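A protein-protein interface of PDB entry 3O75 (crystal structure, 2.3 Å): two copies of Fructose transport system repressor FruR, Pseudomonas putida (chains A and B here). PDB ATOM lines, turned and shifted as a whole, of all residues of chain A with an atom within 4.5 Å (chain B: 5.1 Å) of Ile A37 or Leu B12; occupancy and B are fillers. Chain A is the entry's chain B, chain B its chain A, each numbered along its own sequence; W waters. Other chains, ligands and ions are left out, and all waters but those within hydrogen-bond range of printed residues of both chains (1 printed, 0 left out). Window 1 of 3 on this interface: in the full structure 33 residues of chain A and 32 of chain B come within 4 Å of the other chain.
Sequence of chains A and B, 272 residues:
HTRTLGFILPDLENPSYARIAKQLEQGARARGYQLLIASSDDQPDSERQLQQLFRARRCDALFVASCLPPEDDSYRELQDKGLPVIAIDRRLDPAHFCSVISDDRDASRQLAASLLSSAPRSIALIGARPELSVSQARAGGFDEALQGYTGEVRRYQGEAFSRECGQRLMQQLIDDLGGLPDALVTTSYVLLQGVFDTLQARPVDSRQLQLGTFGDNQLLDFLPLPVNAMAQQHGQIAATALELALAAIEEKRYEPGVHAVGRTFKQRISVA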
ATOM      1  N   PHE A   7      -0.641  23.214   6.299  1.00  0.00           N
ATOM      2  CA  PHE A   7      -0.002  24.406   6.847  1.00  0.00           C
ATOM      3  C   PHE A   7      -0.771  24.927   8.060  1.00  0.00           C
ATOM      4  O   PHE A   7      -1.885  25.433   7.932  1.00  0.00           O
ATOM      5  CB  PHE A   7       0.116  25.496   5.776  1.00  0.00           C
ATOM      6  CG  PHE A   7       0.888  26.714   6.219  1.00  0.00           C
ATOM      7  CD1 PHE A   7       1.800  26.640   7.266  1.00  0.00           C
ATOM      8  CD2 PHE A   7       0.713  27.930   5.578  1.00  0.00           C
ATOM      9  CE1 PHE A   7       2.515  27.757   7.671  1.00  0.00           C
ATOM     10  CE2 PHE A   7       1.427  29.052   5.974  1.00  0.00           C
ATOM     11  CZ  PHE A   7       2.327  28.968   7.022  1.00  0.00           C
ATOM     12  N   LEU A   9      -0.990  27.731  10.684  1.00  0.00           N
ATOM     13  CA  LEU A   9      -0.528  29.093  10.939  1.00  0.00           C
ATOM     14  C   LEU A   9      -1.303  29.712  12.094  1.00  0.00           C
ATOM     15  O   LEU A   9      -2.399  29.251  12.417  1.00  0.00           O
ATOM     16  CB  LEU A   9      -0.600  29.953   9.668  1.00  0.00           C
ATOM     17  CG  LEU A   9      -1.900  30.000   8.861  1.00  0.00           C
ATOM     18  CD1 LEU A   9      -2.854  31.008   9.466  1.00  0.00           C
ATOM     19  CD2 LEU A   9      -1.601  30.360   7.416  1.00  0.00           C
ATOM     20  N   ALA A  18      -0.679  35.062   5.437  1.00  0.00           N
ATOM     21  CA  ALA A  18      -1.485  34.826   4.244  1.00  0.00           C
ATOM     22  C   ALA A  18      -0.597  34.873   3.011  1.00  0.00           C
ATOM     23  O   ALA A  18      -0.764  34.092   2.078  1.00  0.00           O
ATOM     24  CB  ALA A  18      -2.604  35.860   4.135  1.00  0.00           C
ATOM     25  N   ALA A  21       1.391  31.660   3.047  1.00  0.00           N
ATOM     26  CA  ALA A  21       0.472  30.587   2.671  1.00  0.00           C
ATOM     27  C   ALA A  21       0.169  30.607   1.171  1.00  0.00           C
ATOM     28  O   ALA A  21       0.215  29.574   0.508  1.00  0.00           O
ATOM     29  CB  ALA A  21      -0.826  30.673   3.480  1.00  0.00           C
ATOM     30  N   LYS A  22      -0.144  31.784   0.641  1.00  0.00           N
ATOM     31  CA  LYS A  22      -0.427  31.908  -0.783  1.00  0.00           C
ATOM     32  C   LYS A  22       0.785  31.465  -1.593  1.00  0.00           C
ATOM     33  O   LYS A  22       0.656  30.774  -2.606  1.00  0.00           O
ATOM     34  CB  LYS A  22      -0.798  33.348  -1.142  1.00  0.00           C
ATOM     35  CG  LYS A  22      -1.085  33.545  -2.626  1.00  0.00           C
ATOM     36  CD  LYS A  22      -1.789  34.868  -2.891  1.00  0.00           C
ATOM     37  CE  LYS A  22      -2.121  35.021  -4.368  1.00  0.00           C
ATOM     38  NZ  LYS A  22      -2.914  36.251  -4.633  1.00  0.00           N
ATOM     39  N   GLU A  25       1.182  27.779  -1.412  1.00  0.00           N
ATOM     40  CA  GLU A  25       0.111  27.239  -2.238  1.00  0.00           C
ATOM     41  C   GLU A  25       0.450  27.246  -3.731  1.00  0.00           C
ATOM     42  O   GLU A  25       0.281  26.239  -4.416  1.00  0.00           O
ATOM     43  CB  GLU A  25      -1.168  28.038  -1.992  1.00  0.00           C
ATOM     44  CG  GLU A  25      -2.219  27.891  -3.064  1.00  0.00           C
ATOM     45  CD  GLU A  25      -2.963  29.186  -3.314  1.00  0.00           C
ATOM     46  OE1 GLU A  25      -2.821  30.128  -2.505  1.00  0.00           O
ATOM     47  OE2 GLU A  25      -3.685  29.263  -4.324  1.00  0.00           O
ATOM     48  N   LEU A  35      -2.581  22.402  -1.165  1.00  0.00           N
ATOM     49  CA  LEU A  35      -2.322  22.881   0.189  1.00  0.00           C
ATOM     50  C   LEU A  35      -3.605  23.049   0.998  1.00  0.00           C
ATOM     51  O   LEU A  35      -4.557  23.699   0.550  1.00  0.00           O
ATOM     52  CB  LEU A  35      -1.547  24.204   0.152  1.00  0.00           C
ATOM     53  CG  LEU A  35      -1.128  24.813   1.495  1.00  0.00           C
ATOM     54  CD1 LEU A  35      -0.196  23.880   2.239  1.00  0.00           C
ATOM     55  CD2 LEU A  35      -0.463  26.159   1.288  1.00  0.00           C
ATOM     56  N   LEU A  36      -3.625  22.452   2.187  1.00  0.00           N
ATOM     57  CA  LEU A  36      -4.734  22.635   3.115  1.00  0.00           C
ATOM     58  C   LEU A  36      -4.267  23.475   4.298  1.00  0.00           C
ATOM     59  O   LEU A  36      -3.303  23.121   4.982  1.00  0.00           O
ATOM     60  CB  LEU A  36      -5.270  21.289   3.597  1.00  0.00           C
ATOM     61  CG  LEU A  36      -5.899  20.394   2.531  1.00  0.00           C
ATOM     62  CD1 LEU A  36      -6.015  18.960   3.025  1.00  0.00           C
ATOM     63  CD2 LEU A  36      -7.250  20.937   2.127  1.00  0.00           C
ATOM     64  N   ILE A  37      -4.964  24.580   4.537  1.00  0.00           N
ATOM     65  CA  ILE A  37      -4.536  25.568   5.515  1.00  0.00           C
ATOM     66  C   ILE A  37      -5.463  25.619   6.727  1.00  0.00           C
ATOM     67  O   ILE A  37      -6.681  25.518   6.598  1.00  0.00           O
ATOM     68  CB  ILE A  37      -4.462  26.963   4.868  1.00  0.00           C
ATOM     69  CG1 ILE A  37      -3.549  26.925   3.640  1.00  0.00           C
ATOM     70  CG2 ILE A  37      -3.979  27.996   5.867  1.00  0.00           C
ATOM     71  CD1 ILE A  37      -3.539  28.200   2.845  1.00  0.00           C
ATOM     72  N   ALA A  38      -4.880  25.780   7.909  1.00  0.00           N
ATOM     73  CA  ALA A  38      -5.666  25.914   9.129  1.00  0.00           C
ATOM     74  C   ALA A  38      -4.953  26.817  10.115  1.00  0.00           C
ATOM     75  O   ALA A  38      -3.730  26.958  10.070  1.00  0.00           O
ATOM     76  CB  ALA A  38      -5.940  24.559   9.753  1.00  0.00           C
ATOM     77  N   LEU B   9     -11.825  29.526  -1.000  1.00  0.00           N
ATOM     78  CA  LEU B   9     -11.846  30.962  -1.249  1.00  0.00           C
ATOM     79  C   LEU B   9     -10.922  31.289  -2.418  1.00  0.00           C
ATOM     80  O   LEU B   9     -10.017  30.516  -2.728  1.00  0.00           O
ATOM     81  CB  LEU B   9     -11.442  31.735   0.012  1.00  0.00           C
ATOM     82  CG  LEU B   9     -10.131  31.343   0.702  1.00  0.00           C
ATOM     83  CD1 LEU B   9      -8.934  31.975   0.003  1.00  0.00           C
ATOM     84  CD2 LEU B   9     -10.161  31.748   2.166  1.00  0.00           C
ATOM     85  N   PRO B  10     -11.165  32.427  -3.084  1.00  0.00           N
ATOM     86  CA  PRO B  10     -10.428  32.832  -4.288  1.00  0.00           C
ATOM     87  C   PRO B  10      -9.022  33.397  -4.035  1.00  0.00           C
ATOM     88  O   PRO B  10      -8.132  33.165  -4.850  1.00  0.00           O
ATOM     89  CB  PRO B  10     -11.313  33.936  -4.888  1.00  0.00           C
ATOM     90  CG  PRO B  10     -12.621  33.853  -4.164  1.00  0.00           C
ATOM     91  CD  PRO B  10     -12.296  33.328  -2.812  1.00  0.00           C
ATOM     92  N   ASP B  11      -8.823  34.132  -2.943  1.00  0.00           N
ATOM     93  CA  ASP B  11      -7.567  34.856  -2.747  1.00  0.00           C
ATOM     94  C   ASP B  11      -7.204  35.032  -1.275  1.00  0.00           C
ATOM     95  O   ASP B  11      -7.858  35.777  -0.542  1.00  0.00           O
ATOM     96  CB  ASP B  11      -7.634  36.223  -3.439  1.00  0.00           C
ATOM     97  CG  ASP B  11      -6.297  36.956  -3.432  1.00  0.00           C
ATOM     98  OD1 ASP B  11      -5.280  36.363  -3.016  1.00  0.00           O
ATOM     99  OD2 ASP B  11      -6.259  38.132  -3.850  1.00  0.00           O
ATOM    100  N   LEU B  12      -6.141  34.347  -0.864  1.00  0.00           N
ATOM    101  CA  LEU B  12      -5.639  34.407   0.501  1.00  0.00           C
ATOM    102  C   LEU B  12      -5.139  35.799   0.858  1.00  0.00           C
ATOM    103  O   LEU B  12      -5.156  36.190   2.023  1.00  0.00           O
ATOM    104  CB  LEU B  12      -4.515  33.384   0.690  1.00  0.00           C
ATOM    105  CG  LEU B  12      -4.952  31.916   0.651  1.00  0.00           C
ATOM    106  CD1 LEU B  12      -3.795  30.979   0.310  1.00  0.00           C
ATOM    107  CD2 LEU B  12      -5.601  31.528   1.969  1.00  0.00           C
ATOM    108  N   GLU B  13      -4.685  36.544  -0.144  1.00  0.00           N
ATOM    109  CA  GLU B  13      -4.175  37.893   0.092  1.00  0.00           C
ATOM    110  C   GLU B  13      -5.230  38.985  -0.094  1.00  0.00           C
ATOM    111  O   GLU B  13      -4.904  40.174  -0.120  1.00  0.00           O
ATOM    112  CB  GLU B  13      -2.943  38.183  -0.768  1.00  0.00           C
ATOM    113  CG  GLU B  13      -1.734  37.347  -0.415  1.00  0.00           C
ATOM    114  CD  GLU B  13      -0.423  38.007  -0.811  1.00  0.00           C
ATOM    115  OE1 GLU B  13      -0.166  39.148  -0.369  1.00  0.00           O
ATOM    116  OE2 GLU B  13       0.362  37.379  -1.552  1.00  0.00           O
ATOM    117  N   ASN B  14      -6.487  38.580  -0.247  1.00  0.00           N
ATOM    118  CA  ASN B  14      -7.599  39.515  -0.140  1.00  0.00           C
ATOM    119  C   ASN B  14      -8.082  39.496   1.305  1.00  0.00           C
ATOM    120  O   ASN B  14      -8.674  38.514   1.751  1.00  0.00           O
ATOM    121  CB  ASN B  14      -8.730  39.130  -1.094  1.00  0.00           C
ATOM    122  CG  ASN B  14      -9.833  40.182  -1.158  1.00  0.00           C
ATOM    123  OD1 ASN B  14     -10.289  40.690  -0.132  1.00  0.00           O
ATOM    124  ND2 ASN B  14     -10.271  40.505  -2.371  1.00  0.00           N
ATOM    125  N   ALA B  18      -9.636  36.448   4.088  1.00  0.00           N
ATOM    126  CA  ALA B  18      -8.897  36.055   5.280  1.00  0.00           C
ATOM    127  C   ALA B  18      -9.760  36.317   6.511  1.00  0.00           C
ATOM    128  O   ALA B  18      -9.782  35.528   7.456  1.00  0.00           O
ATOM    129  CB  ALA B  18      -7.603  36.837   5.372  1.00  0.00           C
ATOM    130  N   LEU B  35     -11.715  23.841  10.826  1.00  0.00           N
ATOM    131  CA  LEU B  35     -11.871  24.420   9.493  1.00  0.00           C
ATOM    132  C   LEU B  35     -10.605  24.305   8.648  1.00  0.00           C
ATOM    133  O   LEU B  35      -9.546  24.823   9.017  1.00  0.00           O
ATOM    134  CB  LEU B  35     -12.284  25.893   9.586  1.00  0.00           C
ATOM    135  CG  LEU B  35     -12.508  26.624   8.254  1.00  0.00           C
ATOM    136  CD1 LEU B  35     -13.674  26.017   7.473  1.00  0.00           C
ATOM    137  CD2 LEU B  35     -12.734  28.112   8.467  1.00  0.00           C
ATOM    138  N   LEU B  36     -10.732  23.632   7.509  1.00  0.00           N
ATOM    139  CA  LEU B  36      -9.650  23.534   6.537  1.00  0.00           C
ATOM    140  C   LEU B  36      -9.891  24.477   5.364  1.00  0.00           C
ATOM    141  O   LEU B  36     -10.949  24.447   4.736  1.00  0.00           O
ATOM    142  CB  LEU B  36      -9.529  22.102   6.025  1.00  0.00           C
ATOM    143  CG  LEU B  36      -9.028  21.070   7.033  1.00  0.00           C
ATOM    144  CD1 LEU B  36      -8.951  19.706   6.380  1.00  0.00           C
ATOM    145  CD2 LEU B  36      -7.671  21.485   7.555  1.00  0.00           C
ATOM    146  N   ILE B  37      -8.895  25.297   5.059  1.00  0.00           N
ATOM    147  CA  ILE B  37      -9.032  26.337   4.053  1.00  0.00           C
ATOM    148  C   ILE B  37      -8.144  26.052   2.845  1.00  0.00           C
ATOM    149  O   ILE B  37      -7.040  25.534   2.990  1.00  0.00           O
ATOM    150  CB  ILE B  37      -8.645  27.692   4.655  1.00  0.00           C
ATOM    151  CG1 ILE B  37      -9.530  28.005   5.863  1.00  0.00           C
ATOM    152  CG2 ILE B  37      -8.727  28.793   3.615  1.00  0.00           C
ATOM    153  CD1 ILE B  37      -8.930  29.026   6.795  1.00  0.00           C
ATOM    154  N   ALA B  38      -8.631  26.389   1.655  1.00  0.00           N
ATOM    155  CA  ALA B  38      -7.838  26.237   0.441  1.00  0.00           C
ATOM    156  C   ALA B  38      -8.210  27.318  -0.562  1.00  0.00           C
ATOM    157  O   ALA B  38      -9.349  27.770  -0.594  1.00  0.00           O
ATOM    158  CB  ALA B  38      -8.041  24.858  -0.168  1.00  0.00           C
ATOM    159  N   SER B  39      -7.242  27.727  -1.377  1.00  0.00           N
ATOM    160  CA  SER B  39      -7.435  28.819  -2.327  1.00  0.00           C
ATOM    161  C   SER B  39      -7.516  28.344  -3.776  1.00  0.00           C
ATOM    162  O   SER B  39      -6.841  27.392  -4.166  1.00  0.00           O
ATOM    163  CB  SER B  39      -6.308  29.842  -2.184  1.00  0.00           C
ATOM    164  OG  SER B  39      -6.336  30.777  -3.245  1.00  0.00           O
HETATM  165  O   HOH W   1      -4.604  32.883  -2.837  1.00  0.00           O
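N of Ile B37 is in hydrogen-bond range of O of Ile A37, at 2.7 Å. OD1 of Asp B11 is in salt-bridge range of NZ of Lys A22 (2.9 Å). OE2 of Glu A25 sits at hydrogen-bond distance from OG of Ser B39.
Of the printed residues of chain B, Ala A18 touches Leu B12 (3.3 Å). Of the printed residues of chain B, Lys A22 touches Asp B11, Leu B12 and Glu B13. Of the printed residues of chain B, Leu A36 touches Ile B37. Of the printed residues of chain B, Ala A38 touches Leu B35 (3.7 Å). Leu B12 touches just these residues of chain A: Ala A18 (3.3 Å), Lys A22 (3.7 Å), Glu A25 (3.1 Å) and Ile A37 (3.8 Å). Printed residues of chain A within 4 Å of Glu B13: Lys A22 (3.5 Å). The nearest residue of chain B that does not touch Ile A37 is Ala B38 (5.0 Å). The nearest printed residue of chain B that does not touch Glu A25 is Pro B10 (5.9 Å).
Leu A35 touches Ile B37, and with the chains exchanged Ile A37 touches Leu B35. Leu A35 touches Ala B38, and with the chains exchanged Ala A38 touches Leu B35. Leu A36 touches Ile B37, and with the chains exchanged Ile A37 touches Leu B36. Ile A37 touches its own counterpart, Ile B37. Of the 14 pairs that touch across the chains among the printed residues, 7 have their exchanged pair printed and touching as well.
Hydrophobic or aromatic side chains of chain A within 4 Å of the printed part of chain B: Ala A18, Ile A37 and Ala A38. Hydrophobic or aromatic side chains of chain B within 4 Å of the printed part of chain A: Leu B12, Ile B37 and Ala B38.
Water W1 lies within hydrogen-bond range of the side-chain hydroxyl (OG) of Ser B39 (2.8 Å), the backbone NH (N) of Leu B12 (2.9 Å) and the side-chain carboxylate (OE1) of Glu A25 (3.3 Å).
Ala A18 touches Leu B12 (CB to O, 3.3 Å). Leu B12 touches Lys A22 (CD1 to CA, 3.7 Å). Glu B13 touches Lys A22 (CG to CD, 3.5 Å). Leu B12 touches Glu A25 (CD1 to OE1, 3.1 Å). Leu A35 touches Ile B37 (O to O, 3.9 Å). CB of Ala B38 touches O of Leu A35 (3.7 Å). CD1 of Leu B12 touches CD1 of Ile A37 (3.8 Å). O of Leu B35 touches O of Ile A37, at 3.8 Å. Ile A37 touches Leu B36. O of Leu B35 touches CB of Ala A38 (3.7 Å).
The backbone NH (N) of Leu B9 sits at hydrogen-bond distance from the backbone carbonyl oxygen (O) of Ala B38 (3.1 Å). N of Leu A9 is in hydrogen-bond range of O of Ala A38 (2.9 Å). O of Leu A36 sits at hydrogen-bond distance from N of Phe A7, at 3.0 Å. N of Ala A38 is in hydrogen-bond range of O of Phe A7 (3.0 Å). O of Pro B10 lies within hydrogen-bond range of OG of Ser B39, 3.4 Å away. The side-chain carboxylate of Asp B11 is in hydrogen-bond range of the backbone NH of Glu B13 (2.9 Å).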
